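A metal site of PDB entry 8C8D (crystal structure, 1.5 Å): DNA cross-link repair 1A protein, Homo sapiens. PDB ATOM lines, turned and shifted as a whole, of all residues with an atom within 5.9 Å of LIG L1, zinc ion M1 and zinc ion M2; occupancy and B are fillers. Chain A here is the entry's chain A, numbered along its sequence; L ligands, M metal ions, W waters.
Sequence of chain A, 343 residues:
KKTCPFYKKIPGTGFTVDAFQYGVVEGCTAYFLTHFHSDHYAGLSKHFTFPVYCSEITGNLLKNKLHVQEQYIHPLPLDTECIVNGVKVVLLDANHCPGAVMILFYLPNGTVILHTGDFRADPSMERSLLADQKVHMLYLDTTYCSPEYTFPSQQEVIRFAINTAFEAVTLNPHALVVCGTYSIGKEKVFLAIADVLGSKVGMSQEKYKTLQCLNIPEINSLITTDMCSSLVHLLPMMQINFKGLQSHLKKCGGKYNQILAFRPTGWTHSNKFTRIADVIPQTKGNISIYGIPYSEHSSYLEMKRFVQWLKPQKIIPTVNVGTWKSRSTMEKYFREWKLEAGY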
ATOM      1  N   HIS A  35       5.811  21.659  -6.616  1.00  0.00           N
ATOM      2  CA  HIS A  35       5.197  20.449  -6.097  1.00  0.00           C
ATOM      3  C   HIS A  35       5.324  20.404  -4.579  1.00  0.00           C
ATOM      4  O   HIS A  35       6.138  21.118  -3.990  1.00  0.00           O
ATOM      5  CB  HIS A  35       5.748  19.164  -6.748  1.00  0.00           C
ATOM      6  CG  HIS A  35       7.187  18.859  -6.457  1.00  0.00           C
ATOM      7  ND1 HIS A  35       8.240  19.642  -6.902  1.00  0.00           N
ATOM      8  CD2 HIS A  35       7.753  17.812  -5.817  1.00  0.00           C
ATOM      9  CE1 HIS A  35       9.380  19.102  -6.530  1.00  0.00           C
ATOM     10  NE2 HIS A  35       9.111  17.976  -5.872  1.00  0.00           N
ATOM     11  N   HIS A  37       6.714  18.724  -2.083  1.00  0.00           N
ATOM     12  CA  HIS A  37       7.787  17.979  -1.430  1.00  0.00           C
ATOM     13  C   HIS A  37       8.548  18.924  -0.510  1.00  0.00           C
ATOM     14  O   HIS A  37       8.767  20.087  -0.856  1.00  0.00           O
ATOM     15  CB  HIS A  37       8.752  17.347  -2.441  1.00  0.00           C
ATOM     16  CG  HIS A  37       8.289  16.034  -2.989  1.00  0.00           C
ATOM     17  ND1 HIS A  37       8.821  15.478  -4.122  1.00  0.00           N
ATOM     18  CD2 HIS A  37       7.340  15.166  -2.552  1.00  0.00           C
ATOM     19  CE1 HIS A  37       8.229  14.320  -4.363  1.00  0.00           C
ATOM     20  NE2 HIS A  37       7.326  14.107  -3.427  1.00  0.00           N
ATOM     21  N   SER A  38       8.977  18.411   0.645  1.00  0.00           N
ATOM     22  CA  SER A  38       9.436  19.283   1.725  1.00  0.00           C
ATOM     23  C   SER A  38      10.661  20.112   1.343  1.00  0.00           C
ATOM     24  O   SER A  38      10.802  21.250   1.819  1.00  0.00           O
ATOM     25  CB  SER A  38       9.694  18.479   3.005  1.00  0.00           C
ATOM     26  OG  SER A  38      10.651  17.464   2.785  1.00  0.00           O
ATOM     27  N   ASP A  39      11.538  19.584   0.489  1.00  0.00           N
ATOM     28  CA  ASP A  39      12.688  20.352   0.038  1.00  0.00           C
ATOM     29  C   ASP A  39      12.301  21.511  -0.883  1.00  0.00           C
ATOM     30  O   ASP A  39      13.174  22.313  -1.245  1.00  0.00           O
ATOM     31  CB  ASP A  39      13.746  19.459  -0.623  1.00  0.00           C
ATOM     32  CG  ASP A  39      13.152  18.473  -1.611  1.00  0.00           C
ATOM     33  OD1 ASP A  39      12.069  17.913  -1.312  1.00  0.00           O
ATOM     34  OD2 ASP A  39      13.759  18.253  -2.678  1.00  0.00           O
ATOM     35  N   HIS A  40      11.028  21.622  -1.241  1.00  0.00           N
ATOM     36  CA  HIS A  40      10.550  22.689  -2.108  1.00  0.00           C
ATOM     37  C   HIS A  40       9.598  23.655  -1.418  1.00  0.00           C
ATOM     38  O   HIS A  40       9.661  24.861  -1.681  1.00  0.00           O
ATOM     39  CB  HIS A  40       9.891  22.112  -3.362  1.00  0.00           C
ATOM     40  CG  HIS A  40      10.824  21.225  -4.133  1.00  0.00           C
ATOM     41  ND1 HIS A  40      11.467  21.646  -5.281  1.00  0.00           N
ATOM     42  CD2 HIS A  40      11.265  19.969  -3.899  1.00  0.00           C
ATOM     43  CE1 HIS A  40      12.244  20.688  -5.723  1.00  0.00           C
ATOM     44  NE2 HIS A  40      12.136  19.649  -4.901  1.00  0.00           N
ATOM     45  N   HIS A  96       6.391  13.673 -12.063  1.00  0.00           N
ATOM     46  CA  HIS A  96       7.117  13.487 -10.804  1.00  0.00           C
ATOM     47  C   HIS A  96       6.115  12.875  -9.824  1.00  0.00           C
ATOM     48  O   HIS A  96       5.739  11.711  -9.986  1.00  0.00           O
ATOM     49  CB  HIS A  96       7.723  14.833 -10.363  1.00  0.00           C
ATOM     50  CG  HIS A  96       8.588  14.779  -9.140  1.00  0.00           C
ATOM     51  ND1 HIS A  96       9.663  13.916  -8.999  1.00  0.00           N
ATOM     52  CD2 HIS A  96       8.565  15.524  -8.005  1.00  0.00           C
ATOM     53  CE1 HIS A  96      10.246  14.135  -7.830  1.00  0.00           C
ATOM     54  NE2 HIS A  96       9.599  15.094  -7.207  1.00  0.00           N
ATOM     55  N   CYS A  97       5.660  13.630  -8.849  1.00  0.00           N
ATOM     56  CA  CYS A  97       4.631  13.193  -7.902  1.00  0.00           C
ATOM     57  C   CYS A  97       3.302  13.869  -8.239  1.00  0.00           C
ATOM     58  O   CYS A  97       3.251  14.766  -9.084  1.00  0.00           O
ATOM     59  CB  CYS A  97       5.056  13.556  -6.481  1.00  0.00           C
ATOM     60  SG  CYS A  97       5.151  15.331  -6.174  1.00  0.00           S
ATOM     61  N   ASP A 118      10.997  19.424 -10.145  1.00  0.00           N
ATOM     62  CA  ASP A 118      11.482  18.049 -10.224  1.00  0.00           C
ATOM     63  C   ASP A 118      10.692  17.334 -11.319  1.00  0.00           C
ATOM     64  O   ASP A 118       9.462  17.486 -11.375  1.00  0.00           O
ATOM     65  CB  ASP A 118      11.255  17.299  -8.906  1.00  0.00           C
ATOM     66  CG  ASP A 118      12.247  17.679  -7.834  1.00  0.00           C
ATOM     67  OD1 ASP A 118      13.204  18.433  -8.109  1.00  0.00           O
ATOM     68  OD2 ASP A 118      12.053  17.212  -6.687  1.00  0.00           O
ATOM     69  N   THR A 143      19.105  15.950 -10.741  1.00  0.00           N
ATOM     70  CA  THR A 143      19.336  15.010  -9.639  1.00  0.00           C
ATOM     71  C   THR A 143      20.254  13.863 -10.067  1.00  0.00           C
ATOM     72  O   THR A 143      21.241  13.575  -9.394  1.00  0.00           O
ATOM     73  CB  THR A 143      17.995  14.475  -9.097  1.00  0.00           C
ATOM     74  OG1 THR A 143      17.211  15.568  -8.618  1.00  0.00           O
ATOM     75  CG2 THR A 143      18.233  13.478  -7.961  1.00  0.00           C
ATOM     76  N   TYR A 144      19.951  13.229 -11.183  1.00  0.00           N
ATOM     77  CA  TYR A 144      20.704  12.052 -11.630  1.00  0.00           C
ATOM     78  C   TYR A 144      21.507  12.313 -12.899  1.00  0.00           C
ATOM     79  O   TYR A 144      21.571  11.469 -13.797  1.00  0.00           O
ATOM     80  CB  TYR A 144      19.777  10.855 -11.798  1.00  0.00           C
ATOM     81  CG  TYR A 144      19.199  10.371 -10.493  1.00  0.00           C
ATOM     82  CD1 TYR A 144      20.001  10.118  -9.405  1.00  0.00           C
ATOM     83  CD2 TYR A 144      17.828  10.184 -10.359  1.00  0.00           C
ATOM     84  CE1 TYR A 144      19.488   9.664  -8.208  1.00  0.00           C
ATOM     85  CE2 TYR A 144      17.292   9.736  -9.159  1.00  0.00           C
ATOM     86  CZ  TYR A 144      18.133   9.478  -8.086  1.00  0.00           C
ATOM     87  OH  TYR A 144      17.618   9.033  -6.891  1.00  0.00           O
ATOM     88  N   TYR A 182       6.855   8.283   2.833  1.00  0.00           N
ATOM     89  CA  TYR A 182       6.929   9.515   3.607  1.00  0.00           C
ATOM     90  C   TYR A 182       6.191  10.623   2.867  1.00  0.00           C
ATOM     91  O   TYR A 182       5.097  11.043   3.271  1.00  0.00           O
ATOM     92  CB  TYR A 182       8.368   9.948   3.926  1.00  0.00           C
ATOM     93  CG  TYR A 182       9.464   9.393   3.039  1.00  0.00           C
ATOM     94  CD1 TYR A 182       9.364   9.405   1.650  1.00  0.00           C
ATOM     95  CD2 TYR A 182      10.646   8.901   3.599  1.00  0.00           C
ATOM     96  CE1 TYR A 182      10.373   8.907   0.855  1.00  0.00           C
ATOM     97  CE2 TYR A 182      11.661   8.404   2.811  1.00  0.00           C
ATOM     98  CZ  TYR A 182      11.524   8.412   1.439  1.00  0.00           C
ATOM     99  OH  TYR A 182      12.533   7.914   0.643  1.00  0.00           O
ATOM    100  N   SER A 183       6.775  11.092   1.779  1.00  0.00           N
ATOM    101  CA  SER A 183       6.177  12.169   1.003  1.00  0.00           C
ATOM    102  C   SER A 183       5.098  11.609   0.092  1.00  0.00           C
ATOM    103  O   SER A 183       4.866  10.397   0.010  1.00  0.00           O
ATOM    104  CB  SER A 183       7.265  12.876   0.190  1.00  0.00           C
ATOM    105  OG  SER A 183       8.002  11.947  -0.575  1.00  0.00           O
ATOM    106  N   ILE A 184       4.416  12.506  -0.616  1.00  0.00           N
ATOM    107  CA  ILE A 184       3.565  12.096  -1.724  1.00  0.00           C
ATOM    108  C   ILE A 184       4.459  11.603  -2.843  1.00  0.00           C
ATOM    109  O   ILE A 184       5.675  11.832  -2.830  1.00  0.00           O
ATOM    110  CB  ILE A 184       2.646  13.233  -2.205  1.00  0.00           C
ATOM    111  CG1 ILE A 184       3.502  14.392  -2.730  1.00  0.00           C
ATOM    112  CG2 ILE A 184       1.719  13.669  -1.085  1.00  0.00           C
ATOM    113  CD1 ILE A 184       2.706  15.483  -3.448  1.00  0.00           C
ATOM    114  N   LYS A 186       4.891   8.093  -5.805  1.00  0.00           N
ATOM    115  CA  LYS A 186       5.094   6.645  -5.829  1.00  0.00           C
ATOM    116  C   LYS A 186       3.872   5.881  -5.323  1.00  0.00           C
ATOM    117  O   LYS A 186       3.993   4.722  -4.918  1.00  0.00           O
ATOM    118  CB  LYS A 186       6.368   6.241  -5.079  1.00  0.00           C
ATOM    119  CG  LYS A 186       7.593   7.087  -5.492  1.00  0.00           C
ATOM    120  CD  LYS A 186       8.897   6.593  -4.859  1.00  0.00           C
ATOM    121  CE  LYS A 186      10.061   7.537  -5.210  1.00  0.00           C
ATOM    122  NZ  LYS A 186      11.363   6.996  -4.731  1.00  0.00           N
ATOM    123  N   THR A 265      12.911   2.990  -3.103  1.00  0.00           N
ATOM    124  CA  THR A 265      14.012   3.947  -3.063  1.00  0.00           C
ATOM    125  C   THR A 265      14.187   4.612  -4.423  1.00  0.00           C
ATOM    126  O   THR A 265      13.485   4.324  -5.393  1.00  0.00           O
ATOM    127  CB  THR A 265      15.302   3.228  -2.698  1.00  0.00           C
ATOM    128  OG1 THR A 265      15.681   2.366  -3.782  1.00  0.00           O
ATOM    129  CG2 THR A 265      15.105   2.394  -1.448  1.00  0.00           C
ATOM    130  N   GLY A 266      15.147   5.534  -4.484  1.00  0.00           N
ATOM    131  CA  GLY A 266      15.601   6.050  -5.765  1.00  0.00           C
ATOM    132  C   GLY A 266      16.669   5.127  -6.336  1.00  0.00           C
ATOM    133  O   GLY A 266      16.567   3.900  -6.205  1.00  0.00           O
ATOM    134  N   TRP A 267      17.692   5.702  -6.952  1.00  0.00           N
ATOM    135  CA  TRP A 267      18.811   4.903  -7.412  1.00  0.00           C
ATOM    136  C   TRP A 267      19.654   4.443  -6.228  1.00  0.00           C
ATOM    137  O   TRP A 267      19.834   5.173  -5.259  1.00  0.00           O
ATOM    138  CB  TRP A 267      19.687   5.711  -8.369  1.00  0.00           C
ATOM    139  CG  TRP A 267      21.012   5.061  -8.715  1.00  0.00           C
ATOM    140  CD1 TRP A 267      21.295   4.293  -9.813  1.00  0.00           C
ATOM    141  CD2 TRP A 267      22.226   5.128  -7.944  1.00  0.00           C
ATOM    142  NE1 TRP A 267      22.611   3.878  -9.773  1.00  0.00           N
ATOM    143  CE2 TRP A 267      23.204   4.380  -8.642  1.00  0.00           C
ATOM    144  CE3 TRP A 267      22.586   5.751  -6.741  1.00  0.00           C
ATOM    145  CZ2 TRP A 267      24.515   4.236  -8.175  1.00  0.00           C
ATOM    146  CZ3 TRP A 267      23.890   5.606  -6.282  1.00  0.00           C
ATOM    147  CH2 TRP A 267      24.828   4.859  -7.000  1.00  0.00           C
ATOM    148  N   HIS A 297      12.439  10.773 -10.678  1.00  0.00           N
ATOM    149  CA  HIS A 297      13.386  11.669 -11.326  1.00  0.00           C
ATOM    150  C   HIS A 297      13.945  11.002 -12.582  1.00  0.00           C
ATOM    151  O   HIS A 297      14.068   9.780 -12.651  1.00  0.00           O
ATOM    152  CB  HIS A 297      14.590  12.016 -10.408  1.00  0.00           C
ATOM    153  CG  HIS A 297      14.237  12.873  -9.228  1.00  0.00           C
ATOM    154  ND1 HIS A 297      14.134  14.244  -9.312  1.00  0.00           N
ATOM    155  CD2 HIS A 297      14.012  12.560  -7.927  1.00  0.00           C
ATOM    156  CE1 HIS A 297      13.844  14.745  -8.121  1.00  0.00           C
ATOM    157  NE2 HIS A 297      13.776  13.737  -7.260  1.00  0.00           N
HETATM  158  C1  LIG L   1      10.541  12.688  -2.472  1.00  0.00           C
HETATM  159  C2  LIG L   1      15.822  15.590  -0.692  1.00  0.00           C
HETATM  160  C3  LIG L   1      15.834  14.257  -2.599  1.00  0.00           C
HETATM  161  C4  LIG L   1      15.946  12.838  -4.614  1.00  0.00           C
HETATM  162  C5  LIG L   1      15.800  11.452  -4.103  1.00  0.00           C
HETATM  163  C6  LIG L   1      16.677  10.603  -3.532  1.00  0.00           C
HETATM  164  C7  LIG L   1      15.964   9.403  -3.234  1.00  0.00           C
HETATM  165  C8  LIG L   1      14.672   9.616  -3.654  1.00  0.00           C
HETATM  166  C9  LIG L   1      11.624  14.585  -3.683  1.00  0.00           C
HETATM  167  C10 LIG L   1      11.849  13.460  -2.673  1.00  0.00           C
HETATM  168  C11 LIG L   1      12.382  14.004  -1.340  1.00  0.00           C
HETATM  169  C12 LIG L   1      13.833  14.412  -1.448  1.00  0.00           C
HETATM  170  C13 LIG L   1      14.452  15.277  -0.489  1.00  0.00           C
HETATM  171  C14 LIG L   1      13.767  15.824   0.610  1.00  0.00           C
HETATM  172  C15 LIG L   1      14.444  16.637   1.474  1.00  0.00           C
HETATM  173  C16 LIG L   1      15.795  16.959   1.296  1.00  0.00           C
HETATM  174  C17 LIG L   1      16.471  16.444   0.221  1.00  0.00           C
HETATM  175  N1  LIG L   1      16.506  15.067  -1.758  1.00  0.00           N
HETATM  176  N2  LIG L   1      16.510  13.757  -3.639  1.00  0.00           N
HETATM  177  N3  LIG L   1      14.529  13.916  -2.478  1.00  0.00           N
HETATM  178  N4  LIG L   1      11.727  15.818  -3.213  1.00  0.00           N
HETATM  179  O1  LIG L   1      14.563  10.874  -4.195  1.00  0.00           O
HETATM  180  O2  LIG L   1      11.484  16.897  -4.057  1.00  0.00           O
HETATM  181  O3  LIG L   1      11.365  14.348  -4.864  1.00  0.00           O
HETATM  182 CL1  LIG L   1      13.615  17.321   2.842  1.00  0.00          CL
HETATM  183  C1  LG2 L   2      13.254  11.791   4.865  1.00  0.00           C
HETATM  184  C2  LG2 L   2      16.486  12.903   1.116  1.00  0.00           C
HETATM  185  C3  LG2 L   2      17.571  14.298   2.642  1.00  0.00           C
HETATM  186  C4  LG2 L   2      18.684  16.214   3.673  1.00  0.00           C
HETATM  187  C5  LG2 L   2      18.395  16.153   5.130  1.00  0.00           C
HETATM  188  C6  LG2 L   2      18.622  15.224   6.065  1.00  0.00           C
HETATM  189  C7  LG2 L   2      18.129  15.746   7.293  1.00  0.00           C
HETATM  190  C8  LG2 L   2      17.644  16.990   7.018  1.00  0.00           C
HETATM  191  C9  LG2 L   2      15.544  12.538   5.520  1.00  0.00           C
HETATM  192  C10 LG2 L   2      14.140  13.005   5.163  1.00  0.00           C
HETATM  193  C11 LG2 L   2      14.160  14.010   3.981  1.00  0.00           C
HETATM  194  C12 LG2 L   2      15.351  13.816   3.076  1.00  0.00           C
HETATM  195  C13 LG2 L   2      15.297  13.011   1.886  1.00  0.00           C
HETATM  196  C14 LG2 L   2      14.140  12.329   1.463  1.00  0.00           C
HETATM  197  C15 LG2 L   2      14.185  11.587   0.324  1.00  0.00           C
HETATM  198  C16 LG2 L   2      15.346  11.474  -0.449  1.00  0.00           C
HETATM  199  C17 LG2 L   2      16.484  12.120  -0.054  1.00  0.00           C
HETATM  200  N1  LG2 L   2      17.631  13.549   1.506  1.00  0.00           N
HETATM  201  N2  LG2 L   2      18.693  14.928   3.015  1.00  0.00           N
HETATM  202  N3  LG2 L   2      16.478  14.433   3.422  1.00  0.00           N
HETATM  203  N4  LG2 L   2      16.164  13.209   6.474  1.00  0.00           N
HETATM  204  O1  LG2 L   2      17.809  17.258   5.684  1.00  0.00           O
HETATM  205  O2  LG2 L   2      15.540  14.275   7.106  1.00  0.00           O
HETATM  206  O3  LG2 L   2      16.048  11.580   4.941  1.00  0.00           O
HETATM  207 CL1  LG2 L   2      12.760  10.745  -0.214  1.00  0.00          CL
HETATM  208 ZN    ZN M   1      13.096  17.770  -4.914  1.00  0.00          ZN
HETATM  209 ZN    ZN M   2      10.239  16.199  -5.500  1.00  0.00          ZN
HETATM  210  O   HOH W   1      14.904   8.895  -6.918  1.00  0.00           O
HETATM  211  O   HOH W   2      14.715  18.452  -6.026  1.00  0.00           O
HETATM  212  O   HOH W   3      14.060  15.807  -4.949  1.00  0.00           O
HETATM  213  O   HOH W   4      11.239  11.578  -5.639  1.00  0.00           O
HETATM  214  O   HOH W   5      16.622  16.253  -5.957  1.00  0.00           O
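O2 of LIG L1 binds zinc ion M1, at 2.0 Å. Water W2 is bound to zinc ion M1, at 2.1 Å. Zinc ion M1 is bound by NE2 of His 40, 2.1 Å away. The side-chain carboxylate (OD2) of Asp 118 binds zinc ion M1. Zinc ion M1 is bound by water W3 (2.2 Å). The side-chain carboxylate (OD2) of Asp 39 binds zinc ion M1, at 2.4 Å.
An oxygen (O3) of LIG L1 sits close to a ring nitrogen (NE2) of His 297 (3.5 Å).
Water W3 lies within hydrogen-bond range of a nitrogen (N4) of LIG L1 (2.9 Å) and a ring nitrogen (NE2) of His 297 (3.1 Å). Water W1 lies within hydrogen-bond range of OH of Tyr 144 and O1 of LIG L1. Water W5 lies within hydrogen-bond range of the side-chain hydroxyl (OG1) of Thr 143 (2.8 Å) and a nitrogen (N2) of LIG L1 (3.4 Å).
Of the 18 residues printed, 3 come within 4 Å of zinc ion M1. Along chain A the residues within 4 Å of zinc ion M1 span positions 39 to 118. The nearest printed residue that does not touch zinc ion M1 is His 35 (4.1 Å).
Zinc ion M2 is bound by O2 of LIG L1 (2.0 Å), ND1 of His 37 (2.1 Å), NE2 of His 96 (2.1 Å), NE2 of His 35 (2.1 Å), O3 of LIG L1 (2.3 Å) and OD2 of Asp 118 (2.4 Å). Zinc ion M2 has six donor atoms within binding distance.
Within 4 Å of zinc ion M2: His 35, His 37, His 40, His 96 and Asp 118. The nearest printed residue that does not touch zinc ion M2 is His 297 (4.7 Å).
OG of Ser 38 touches CL1 of LIG L1, at 3.0 Å. Tyr 144 touches LIG L1. Ser 183 touches LIG L1. Hydrophobic or aromatic side chains within 4 Å of LIG L1: His 35, His 37, His 40, His 96 and His 297. Of the 18 residues printed, 10 come within 4 Å of LIG L1.
NE2 of His 37 sits at hydrogen-bond distance from O of Ile 184, 2.9 Å away. NE2 of His 37 sits close to SG of Cys 97, 3.7 Å away. The side-chain hydroxyl of Thr 143 lies within hydrogen-bond range of a ring nitrogen (ND1) of His 297 (3.4 Å). The backbone NH of Trp 267 lies within hydrogen-bond range of the side-chain hydroxyl of Tyr 144, at 3.3 Å.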
